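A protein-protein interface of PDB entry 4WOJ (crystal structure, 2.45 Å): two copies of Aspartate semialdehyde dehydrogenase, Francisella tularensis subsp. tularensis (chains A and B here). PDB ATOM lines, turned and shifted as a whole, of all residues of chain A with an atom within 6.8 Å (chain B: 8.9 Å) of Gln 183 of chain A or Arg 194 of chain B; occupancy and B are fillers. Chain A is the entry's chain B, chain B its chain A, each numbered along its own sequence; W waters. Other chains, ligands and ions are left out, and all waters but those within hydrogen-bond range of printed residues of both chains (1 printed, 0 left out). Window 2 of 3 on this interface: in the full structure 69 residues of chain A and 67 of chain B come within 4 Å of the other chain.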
ATOM      1  N   ALA A 177     -11.545 -21.502   1.640  1.00  0.00           N
ATOM      2  CA  ALA A 177     -11.188 -20.064   1.536  1.00  0.00           C
ATOM      3  C   ALA A 177      -9.979 -19.752   2.431  1.00  0.00           C
ATOM      4  O   ALA A 177      -9.065 -19.040   2.023  1.00  0.00           O
ATOM      5  CB  ALA A 177     -12.357 -19.189   1.908  1.00  0.00           C
ATOM      6  N   MET A 178      -9.982 -20.323   3.635  1.00  0.00           N
ATOM      7  CA  MET A 178      -8.899 -20.142   4.601  1.00  0.00           C
ATOM      8  C   MET A 178      -7.624 -20.757   4.101  1.00  0.00           C
ATOM      9  O   MET A 178      -6.546 -20.173   4.179  1.00  0.00           O
ATOM     10  CB  MET A 178      -9.255 -20.791   5.923  1.00  0.00           C
ATOM     11  CG  MET A 178      -8.318 -20.404   7.063  1.00  0.00           C
ATOM     12  SD  MET A 178      -9.138 -20.898   8.595  1.00  0.00           S
ATOM     13  CE  MET A 178      -8.302 -20.072   9.908  1.00  0.00           C
ATOM     14  N   GLN A 179      -7.761 -21.969   3.612  1.00  0.00           N
ATOM     15  CA  GLN A 179      -6.636 -22.664   2.995  1.00  0.00           C
ATOM     16  C   GLN A 179      -6.077 -21.811   1.878  1.00  0.00           C
ATOM     17  O   GLN A 179      -4.873 -21.601   1.790  1.00  0.00           O
ATOM     18  CB  GLN A 179      -7.084 -24.019   2.453  1.00  0.00           C
ATOM     19  CG  GLN A 179      -6.989 -25.126   3.477  1.00  0.00           C
ATOM     20  CD  GLN A 179      -7.921 -26.291   3.200  1.00  0.00           C
ATOM     21  OE1 GLN A 179      -8.486 -26.423   2.118  1.00  0.00           O
ATOM     22  NE2 GLN A 179      -8.089 -27.143   4.197  1.00  0.00           N
ATOM     23  N   GLU A 180      -6.960 -21.307   1.028  1.00  0.00           N
ATOM     24  CA  GLU A 180      -6.527 -20.388  -0.039  1.00  0.00           C
ATOM     25  C   GLU A 180      -5.698 -19.222   0.542  1.00  0.00           C
ATOM     26  O   GLU A 180      -4.586 -18.958   0.095  1.00  0.00           O
ATOM     27  CB  GLU A 180      -7.719 -19.877  -0.882  1.00  0.00           C
ATOM     28  CG  GLU A 180      -7.303 -19.586  -2.314  1.00  0.00           C
ATOM     29  CD  GLU A 180      -8.391 -18.968  -3.173  1.00  0.00           C
ATOM     30  OE1 GLU A 180      -8.758 -17.811  -2.901  1.00  0.00           O
ATOM     31  OE2 GLU A 180      -8.871 -19.615  -4.144  1.00  0.00           O
ATOM     32  N   LEU A 181      -6.233 -18.552   1.565  1.00  0.00           N
ATOM     33  CA  LEU A 181      -5.568 -17.385   2.135  1.00  0.00           C
ATOM     34  C   LEU A 181      -4.183 -17.779   2.602  1.00  0.00           C
ATOM     35  O   LEU A 181      -3.190 -17.051   2.345  1.00  0.00           O
ATOM     36  CB  LEU A 181      -6.382 -16.748   3.283  1.00  0.00           C
ATOM     37  CG  LEU A 181      -5.591 -15.777   4.193  1.00  0.00           C
ATOM     38  CD1 LEU A 181      -5.009 -14.591   3.473  1.00  0.00           C
ATOM     39  CD2 LEU A 181      -6.446 -15.285   5.337  1.00  0.00           C
ATOM     40  N   LEU A 182      -4.114 -18.892   3.332  1.00  0.00           N
ATOM     41  CA  LEU A 182      -2.804 -19.380   3.841  1.00  0.00           C
ATOM     42  C   LEU A 182      -1.871 -19.625   2.686  1.00  0.00           C
ATOM     43  O   LEU A 182      -0.717 -19.289   2.739  1.00  0.00           O
ATOM     44  CB  LEU A 182      -2.934 -20.644   4.674  1.00  0.00           C
ATOM     45  CG  LEU A 182      -3.677 -20.501   6.006  1.00  0.00           C
ATOM     46  CD1 LEU A 182      -3.984 -21.868   6.587  1.00  0.00           C
ATOM     47  CD2 LEU A 182      -2.888 -19.641   6.979  1.00  0.00           C
ATOM     48  N   GLN A 183      -2.404 -20.156   1.610  1.00  0.00           N
ATOM     49  CA  GLN A 183      -1.576 -20.493   0.463  1.00  0.00           C
ATOM     50  C   GLN A 183      -1.105 -19.271  -0.337  1.00  0.00           C
ATOM     51  O   GLN A 183       0.071 -19.153  -0.694  1.00  0.00           O
ATOM     52  CB  GLN A 183      -2.333 -21.472  -0.408  1.00  0.00           C
ATOM     53  CG  GLN A 183      -1.823 -21.560  -1.813  1.00  0.00           C
ATOM     54  CD  GLN A 183      -2.025 -22.940  -2.328  1.00  0.00           C
ATOM     55  OE1 GLN A 183      -3.159 -23.391  -2.459  1.00  0.00           O
ATOM     56  NE2 GLN A 183      -0.912 -23.653  -2.579  1.00  0.00           N
ATOM     57  N   GLN A 184      -2.018 -18.365  -0.639  1.00  0.00           N
ATOM     58  CA  GLN A 184      -1.617 -17.082  -1.240  1.00  0.00           C
ATOM     59  C   GLN A 184      -0.411 -16.533  -0.490  1.00  0.00           C
ATOM     60  O   GLN A 184       0.597 -16.215  -1.073  1.00  0.00           O
ATOM     61  CB  GLN A 184      -2.748 -16.064  -1.185  1.00  0.00           C
ATOM     62  CG  GLN A 184      -3.928 -16.404  -2.065  1.00  0.00           C
ATOM     63  CD  GLN A 184      -5.174 -15.604  -1.693  1.00  0.00           C
ATOM     64  OE1 GLN A 184      -5.113 -14.724  -0.818  1.00  0.00           O
ATOM     65  NE2 GLN A 184      -6.328 -15.918  -2.348  1.00  0.00           N
ATOM     66  N   THR A 185      -0.536 -16.455   0.822  1.00  0.00           N
ATOM     67  CA  THR A 185       0.493 -15.869   1.688  1.00  0.00           C
ATOM     68  C   THR A 185       1.813 -16.650   1.645  1.00  0.00           C
ATOM     69  O   THR A 185       2.905 -16.088   1.746  1.00  0.00           O
ATOM     70  CB  THR A 185      -0.023 -15.843   3.137  1.00  0.00           C
ATOM     71  OG1 THR A 185      -1.386 -15.430   3.126  1.00  0.00           O
ATOM     72  CG2 THR A 185       0.775 -14.915   3.993  1.00  0.00           C
ATOM     73  N   SER A 186       1.685 -17.958   1.511  1.00  0.00           N
ATOM     74  CA  SER A 186       2.843 -18.842   1.430  1.00  0.00           C
ATOM     75  C   SER A 186       3.626 -18.573   0.173  1.00  0.00           C
ATOM     76  O   SER A 186       4.829 -18.318   0.227  1.00  0.00           O
ATOM     77  CB  SER A 186       2.414 -20.302   1.462  1.00  0.00           C
ATOM     78  OG  SER A 186       3.486 -21.134   1.025  1.00  0.00           O
ATOM     79  N   LEU A 187       2.926 -18.603  -0.951  1.00  0.00           N
ATOM     80  CA  LEU A 187       3.547 -18.369  -2.262  1.00  0.00           C
ATOM     81  C   LEU A 187       4.203 -16.997  -2.405  1.00  0.00           C
ATOM     82  O   LEU A 187       5.361 -16.897  -2.834  1.00  0.00           O
ATOM     83  CB  LEU A 187       2.517 -18.539  -3.366  1.00  0.00           C
ATOM     84  CG  LEU A 187       1.902 -19.945  -3.470  1.00  0.00           C
ATOM     85  CD1 LEU A 187       0.702 -19.932  -4.407  1.00  0.00           C
ATOM     86  CD2 LEU A 187       2.951 -20.956  -3.939  1.00  0.00           C
ATOM     87  N   LEU A 188       3.471 -15.955  -2.017  1.00  0.00           N
ATOM     88  CA  LEU A 188       4.018 -14.611  -2.002  1.00  0.00           C
ATOM     89  C   LEU A 188       5.235 -14.516  -1.122  1.00  0.00           C
ATOM     90  O   LEU A 188       6.159 -13.767  -1.425  1.00  0.00           O
ATOM     91  CB  LEU A 188       3.009 -13.603  -1.475  1.00  0.00           C
ATOM     92  CG  LEU A 188       1.696 -13.543  -2.193  1.00  0.00           C
ATOM     93  CD1 LEU A 188       0.792 -12.579  -1.452  1.00  0.00           C
ATOM     94  CD2 LEU A 188       1.922 -13.079  -3.599  1.00  0.00           C
ATOM     95  N   SER A 189       5.233 -15.237  -0.011  1.00  0.00           N
ATOM     96  CA  SER A 189       6.398 -15.233   0.886  1.00  0.00           C
ATOM     97  C   SER A 189       7.617 -15.856   0.235  1.00  0.00           C
ATOM     98  O   SER A 189       8.744 -15.455   0.524  1.00  0.00           O
ATOM     99  CB  SER A 189       6.126 -15.975   2.202  1.00  0.00           C
ATOM    100  OG  SER A 189       4.970 -15.485   2.858  1.00  0.00           O
ATOM    101  N   LYS A 190       7.400 -16.852  -0.616  1.00  0.00           N
ATOM    102  CA  LYS A 190       8.527 -17.525  -1.282  1.00  0.00           C
ATOM    103  C   LYS A 190       9.191 -16.590  -2.258  1.00  0.00           C
ATOM    104  O   LYS A 190      10.402 -16.382  -2.182  1.00  0.00           O
ATOM    105  CB  LYS A 190       8.102 -18.806  -1.998  1.00  0.00           C
ATOM    106  CG  LYS A 190       8.115 -19.993  -1.057  1.00  0.00           C
ATOM    107  CD  LYS A 190       7.302 -21.156  -1.583  1.00  0.00           C
ATOM    108  CE  LYS A 190       7.326 -22.296  -0.570  1.00  0.00           C
ATOM    109  NZ  LYS A 190       6.065 -23.078  -0.606  1.00  0.00           N
ATOM    110  N   ILE A 215      -1.107 -17.283  -8.383  1.00  0.00           N
ATOM    111  CA  ILE A 215      -1.648 -17.144  -7.055  1.00  0.00           C
ATOM    112  C   ILE A 215      -3.117 -17.449  -7.076  1.00  0.00           C
ATOM    113  O   ILE A 215      -3.897 -16.644  -7.590  1.00  0.00           O
ATOM    114  CB  ILE A 215      -1.525 -15.681  -6.590  1.00  0.00           C
ATOM    115  CG1 ILE A 215      -0.045 -15.266  -6.501  1.00  0.00           C
ATOM    116  CG2 ILE A 215      -2.238 -15.489  -5.258  1.00  0.00           C
ATOM    117  CD1 ILE A 215       0.833 -16.228  -5.730  1.00  0.00           C
ATOM    118  N   PRO A 216      -3.515 -18.577  -6.484  1.00  0.00           N
ATOM    119  CA  PRO A 216      -4.900 -18.985  -6.546  1.00  0.00           C
ATOM    120  C   PRO A 216      -5.819 -18.030  -5.807  1.00  0.00           C
ATOM    121  O   PRO A 216      -5.571 -17.711  -4.656  1.00  0.00           O
ATOM    122  CB  PRO A 216      -4.892 -20.329  -5.832  1.00  0.00           C
ATOM    123  CG  PRO A 216      -3.822 -20.179  -4.834  1.00  0.00           C
ATOM    124  CD  PRO A 216      -2.759 -19.383  -5.518  1.00  0.00           C
ATOM    125  N   SER B 189       4.850 -18.473   7.447  1.00  0.00           N
ATOM    126  CA  SER B 189       4.559 -19.278   6.245  1.00  0.00           C
ATOM    127  C   SER B 189       5.429 -20.532   6.209  1.00  0.00           C
ATOM    128  O   SER B 189       5.002 -21.564   5.709  1.00  0.00           O
ATOM    129  CB  SER B 189       4.732 -18.485   4.948  1.00  0.00           C
ATOM    130  OG  SER B 189       3.905 -17.331   4.942  1.00  0.00           O
ATOM    131  N   LYS B 190       6.641 -20.447   6.747  1.00  0.00           N
ATOM    132  CA  LYS B 190       7.536 -21.625   6.771  1.00  0.00           C
ATOM    133  C   LYS B 190       7.015 -22.671   7.732  1.00  0.00           C
ATOM    134  O   LYS B 190       6.779 -23.801   7.348  1.00  0.00           O
ATOM    135  CB  LYS B 190       8.969 -21.246   7.137  1.00  0.00           C
ATOM    136  CG  LYS B 190       9.761 -20.777   5.934  1.00  0.00           C
ATOM    137  CD  LYS B 190      10.996 -19.992   6.333  1.00  0.00           C
ATOM    138  CE  LYS B 190      11.734 -19.527   5.087  1.00  0.00           C
ATOM    139  NZ  LYS B 190      12.408 -18.222   5.309  1.00  0.00           N
ATOM    140  N   ILE B 191       6.786 -22.271   8.969  1.00  0.00           N
ATOM    141  CA  ILE B 191       6.260 -23.187   9.973  1.00  0.00           C
ATOM    142  C   ILE B 191       4.906 -23.796   9.599  1.00  0.00           C
ATOM    143  O   ILE B 191       4.611 -24.904  10.006  1.00  0.00           O
ATOM    144  CB  ILE B 191       6.187 -22.519  11.360  1.00  0.00           C
ATOM    145  CG1 ILE B 191       5.856 -23.523  12.473  1.00  0.00           C
ATOM    146  CG2 ILE B 191       5.206 -21.368  11.321  1.00  0.00           C
ATOM    147  CD1 ILE B 191       6.975 -24.511  12.770  1.00  0.00           C
ATOM    148  N   ASP B 192       4.104 -23.109   8.798  1.00  0.00           N
ATOM    149  CA  ASP B 192       2.791 -23.634   8.430  1.00  0.00           C
ATOM    150  C   ASP B 192       2.875 -24.862   7.510  1.00  0.00           C
ATOM    151  O   ASP B 192       3.523 -24.832   6.462  1.00  0.00           O
ATOM    152  CB  ASP B 192       1.950 -22.552   7.763  1.00  0.00           C
ATOM    153  CG  ASP B 192       0.606 -23.055   7.302  1.00  0.00           C
ATOM    154  OD1 ASP B 192      -0.193 -23.547   8.133  1.00  0.00           O
ATOM    155  OD2 ASP B 192       0.345 -22.938   6.092  1.00  0.00           O
ATOM    156  N   ASN B 193       2.163 -25.907   7.922  1.00  0.00           N
ATOM    157  CA  ASN B 193       2.129 -27.202   7.265  1.00  0.00           C
ATOM    158  C   ASN B 193       0.773 -27.475   6.609  1.00  0.00           C
ATOM    159  O   ASN B 193      -0.253 -27.549   7.275  1.00  0.00           O
ATOM    160  CB  ASN B 193       2.416 -28.279   8.315  1.00  0.00           C
ATOM    161  CG  ASN B 193       2.556 -29.668   7.722  1.00  0.00           C
ATOM    162  OD1 ASN B 193       1.805 -30.068   6.824  1.00  0.00           O
ATOM    163  ND2 ASN B 193       3.511 -30.422   8.236  1.00  0.00           N
ATOM    164  N   ARG B 194       0.802 -27.676   5.305  1.00  0.00           N
ATOM    165  CA  ARG B 194      -0.392 -27.959   4.509  1.00  0.00           C
ATOM    166  C   ARG B 194      -1.125 -29.235   4.943  1.00  0.00           C
ATOM    167  O   ARG B 194      -2.349 -29.318   4.855  1.00  0.00           O
ATOM    168  CB  ARG B 194       0.000 -28.109   3.030  1.00  0.00           C
ATOM    169  CG  ARG B 194       1.238 -27.328   2.573  1.00  0.00           C
ATOM    170  CD  ARG B 194       1.341 -27.233   1.056  1.00  0.00           C
ATOM    171  NE  ARG B 194       0.206 -26.477   0.537  1.00  0.00           N
ATOM    172  CZ  ARG B 194      -0.953 -26.998   0.129  1.00  0.00           C
ATOM    173  NH1 ARG B 194      -1.911 -26.187  -0.302  1.00  0.00           N
ATOM    174  NH2 ARG B 194      -1.162 -28.315   0.138  1.00  0.00           N
ATOM    175  N   ASP B 195      -0.365 -30.237   5.367  1.00  0.00           N
ATOM    176  CA  ASP B 195      -0.910 -31.561   5.696  1.00  0.00           C
ATOM    177  C   ASP B 195      -1.616 -31.610   7.032  1.00  0.00           C
ATOM    178  O   ASP B 195      -2.468 -32.470   7.243  1.00  0.00           O
ATOM    179  CB  ASP B 195       0.190 -32.631   5.683  1.00  0.00           C
ATOM    180  CG  ASP B 195       0.663 -32.957   4.282  1.00  0.00           C
ATOM    181  OD1 ASP B 195      -0.164 -32.948   3.333  1.00  0.00           O
ATOM    182  OD2 ASP B 195       1.871 -33.217   4.134  1.00  0.00           O
ATOM    183  N   GLU B 196      -1.272 -30.698   7.928  1.00  0.00           N
ATOM    184  CA  GLU B 196      -1.950 -30.611   9.221  1.00  0.00           C
ATOM    185  C   GLU B 196      -3.420 -30.091   9.079  1.00  0.00           C
ATOM    186  O   GLU B 196      -3.791 -29.462   8.090  1.00  0.00           O
ATOM    187  CB  GLU B 196      -1.122 -29.760  10.181  1.00  0.00           C
ATOM    188  CG  GLU B 196      -1.573 -29.802  11.635  1.00  0.00           C
ATOM    189  CD  GLU B 196      -1.720 -31.212  12.223  1.00  0.00           C
ATOM    190  OE1 GLU B 196      -0.887 -31.622  13.084  1.00  0.00           O
ATOM    191  OE2 GLU B 196      -2.699 -31.904  11.851  1.00  0.00           O
ATOM    192  N   ASP B 197      -4.270 -30.466  10.021  1.00  0.00           N
ATOM    193  CA  ASP B 197      -5.677 -30.042  10.008  1.00  0.00           C
ATOM    194  C   ASP B 197      -5.790 -28.511  10.118  1.00  0.00           C
ATOM    195  O   ASP B 197      -5.054 -27.873  10.878  1.00  0.00           O
ATOM    196  CB  ASP B 197      -6.451 -30.686  11.172  1.00  0.00           C
ATOM    197  CG  ASP B 197      -6.962 -32.104  10.853  1.00  0.00           C
ATOM    198  OD1 ASP B 197      -7.023 -32.510   9.671  1.00  0.00           O
ATOM    199  OD2 ASP B 197      -7.328 -32.817  11.802  1.00  0.00           O
ATOM    200  N   ILE B 198      -6.726 -27.942   9.362  1.00  0.00           N
ATOM    201  CA  ILE B 198      -6.863 -26.471   9.228  1.00  0.00           C
ATOM    202  C   ILE B 198      -6.944 -25.699  10.546  1.00  0.00           C
ATOM    203  O   ILE B 198      -6.300 -24.657  10.683  1.00  0.00           O
ATOM    204  CB  ILE B 198      -8.040 -26.080   8.306  1.00  0.00           C
ATOM    205  CG1 ILE B 198      -7.924 -24.614   7.874  1.00  0.00           C
ATOM    206  CG2 ILE B 198      -9.377 -26.391   8.968  1.00  0.00           C
ATOM    207  CD1 ILE B 198      -6.639 -24.295   7.136  1.00  0.00           C
ATOM    208  N   ARG B 201      -3.527 -25.828  12.247  1.00  0.00           N
ATOM    209  CA  ARG B 201      -2.612 -24.869  11.608  1.00  0.00           C
ATOM    210  C   ARG B 201      -2.812 -23.459  12.149  1.00  0.00           C
ATOM    211  O   ARG B 201      -1.839 -22.770  12.482  1.00  0.00           O
ATOM    212  CB  ARG B 201      -2.805 -24.841  10.105  1.00  0.00           C
ATOM    213  CG  ARG B 201      -2.426 -26.134   9.438  1.00  0.00           C
ATOM    214  CD  ARG B 201      -2.999 -26.239   8.033  1.00  0.00           C
ATOM    215  NE  ARG B 201      -2.357 -25.288   7.131  1.00  0.00           N
ATOM    216  CZ  ARG B 201      -2.666 -25.145   5.849  1.00  0.00           C
ATOM    217  NH1 ARG B 201      -3.612 -25.905   5.296  1.00  0.00           N
ATOM    218  NH2 ARG B 201      -2.046 -24.234   5.121  1.00  0.00           N
ATOM    219  N   LEU B 205       0.057 -21.232  14.082  1.00  0.00           N
ATOM    220  CA  LEU B 205       0.442 -19.853  13.690  1.00  0.00           C
ATOM    221  C   LEU B 205       0.180 -18.928  14.837  1.00  0.00           C
ATOM    222  O   LEU B 205       1.032 -18.130  15.225  1.00  0.00           O
ATOM    223  CB  LEU B 205      -0.348 -19.342  12.493  1.00  0.00           C
ATOM    224  CG  LEU B 205      -0.279 -20.162  11.209  1.00  0.00           C
ATOM    225  CD1 LEU B 205      -1.077 -19.485  10.107  1.00  0.00           C
ATOM    226  CD2 LEU B 205       1.157 -20.372  10.773  1.00  0.00           C
ATOM    227  N   TYR B 226      -1.704 -11.763   9.961  1.00  0.00           N
ATOM    228  CA  TYR B 226      -2.953 -12.400  10.372  1.00  0.00           C
ATOM    229  C   TYR B 226      -3.513 -11.721  11.598  1.00  0.00           C
ATOM    230  O   TYR B 226      -4.124 -12.336  12.452  1.00  0.00           O
ATOM    231  CB  TYR B 226      -2.766 -13.891  10.656  1.00  0.00           C
ATOM    232  CG  TYR B 226      -2.202 -14.679   9.488  1.00  0.00           C
ATOM    233  CD1 TYR B 226      -2.952 -14.907   8.335  1.00  0.00           C
ATOM    234  CD2 TYR B 226      -0.906 -15.206   9.541  1.00  0.00           C
ATOM    235  CE1 TYR B 226      -2.407 -15.643   7.271  1.00  0.00           C
ATOM    236  CE2 TYR B 226      -0.362 -15.915   8.484  1.00  0.00           C
ATOM    237  CZ  TYR B 226      -1.106 -16.145   7.358  1.00  0.00           C
ATOM    238  OH  TYR B 226      -0.523 -16.862   6.334  1.00  0.00           O
HETATM  239  O   HOH W   1       0.701 -20.661   4.569  1.00  0.00           O
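The side-chain hydroxyl (OG) of Ser 189 of chain A is in hydrogen-bond range of the side-chain hydroxyl (OG) of Ser 189 of chain B.
O of Leu 181 of chain A sits at hydrogen-bond distance from OG1 of Thr 185 of chain A, 2.5 Å away. OD2 of Asp 192 of chain B lies within salt-bridge range of NH2 of Arg 201 of chain B. The side-chain hydroxyl of Ser 189 of chain A sits at hydrogen-bond distance from the backbone carbonyl oxygen of Thr 185 of chain A, 2.4 Å away. O of Asn 193 of chain B is in hydrogen-bond range of NE of Arg 201 of chain B.
Ile 198 of chain B touches Met 178 of chain A (CG1 to SD, 3.98 Å). Gln 179 of chain A touches Ile 198 of chain B. Gln 179 of chain A touches Arg 201 of chain B. Leu 182 of chain A touches Arg 201 of chain B. Leu 205 of chain B touches Leu 182 of chain A (CD1 to CD2, 3.6 Å). OH of Tyr 226 of chain B touches CD2 of Leu 182 of chain A (3.7 Å). Gln 183 of chain A touches Arg 194 of chain B (NE2 to NH1, 3.6 Å). O of Thr 185 of chain A touches OG of Ser 189 of chain B (3.6 Å). Tyr 226 of chain B touches Thr 185 of chain A (OH to CG2, 3.3 Å). Ser 189 of chain B touches Ser 186 of chain A (OG to CA, 3.97 Å).
Printed residues of chain B within 4 Å of Gln 183 of chain A: Arg 194 (3.6 Å). Arg 194 of chain B touches one residue of chain A. Of the printed residues of chain A, Ser 189 of chain B touches Thr 185, Ser 186 and Ser 189. Of the printed residues of chain A, Tyr 226 of chain B touches Leu 182 (3.7 Å) and Thr 185 (3.3 Å). Printed residues of chain A within 4 Å of Arg 201 of chain B: Gln 179 and Leu 182. Of the printed residues of chain B, Leu 182 of chain A touches Ile 198 (3.6 Å), Arg 201 (3.4 Å), Leu 205 (3.6 Å) and Tyr 226 (3.7 Å). Leu 181 of chain A touches none of the printed residues of chain B. Ile 215 of chain A touches none of the printed residues of chain B. The nearest residue of chain B that does not touch Gln 183 of chain A is Arg 201 of chain B (5.4 Å). The nearest printed residue of chain B that does not touch Ser 189 of chain A is Lys 190 of chain B (6.4 Å).
Of the 16 printed residues of chain A, 7 touch a printed residue of chain B. Hydrophobic or aromatic side chains of chain A that line the printed part of chain B: Met 178 and Leu 182. Of the 13 printed residues of chain B, 6 touch a printed residue of chain A. Printed residues of chain B that touch a printed residue of chain A: Ser 189, Arg 194, Ile 198, Arg 201, Leu 205 and Tyr 226. Hydrophobic or aromatic side chains of chain B that line the printed part of chain A: Ile 198, Leu 205 and Tyr 226.
Ser 189 of chain B touches its own counterpart, Ser 189 of chain A. Of the 12 pairs that touch across the chains among the printed residues, 1 has its exchanged pair printed and touching as well.
Water W1 bridges O of Leu 182 of chain A and OD2 of Asp 192 of chain B.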
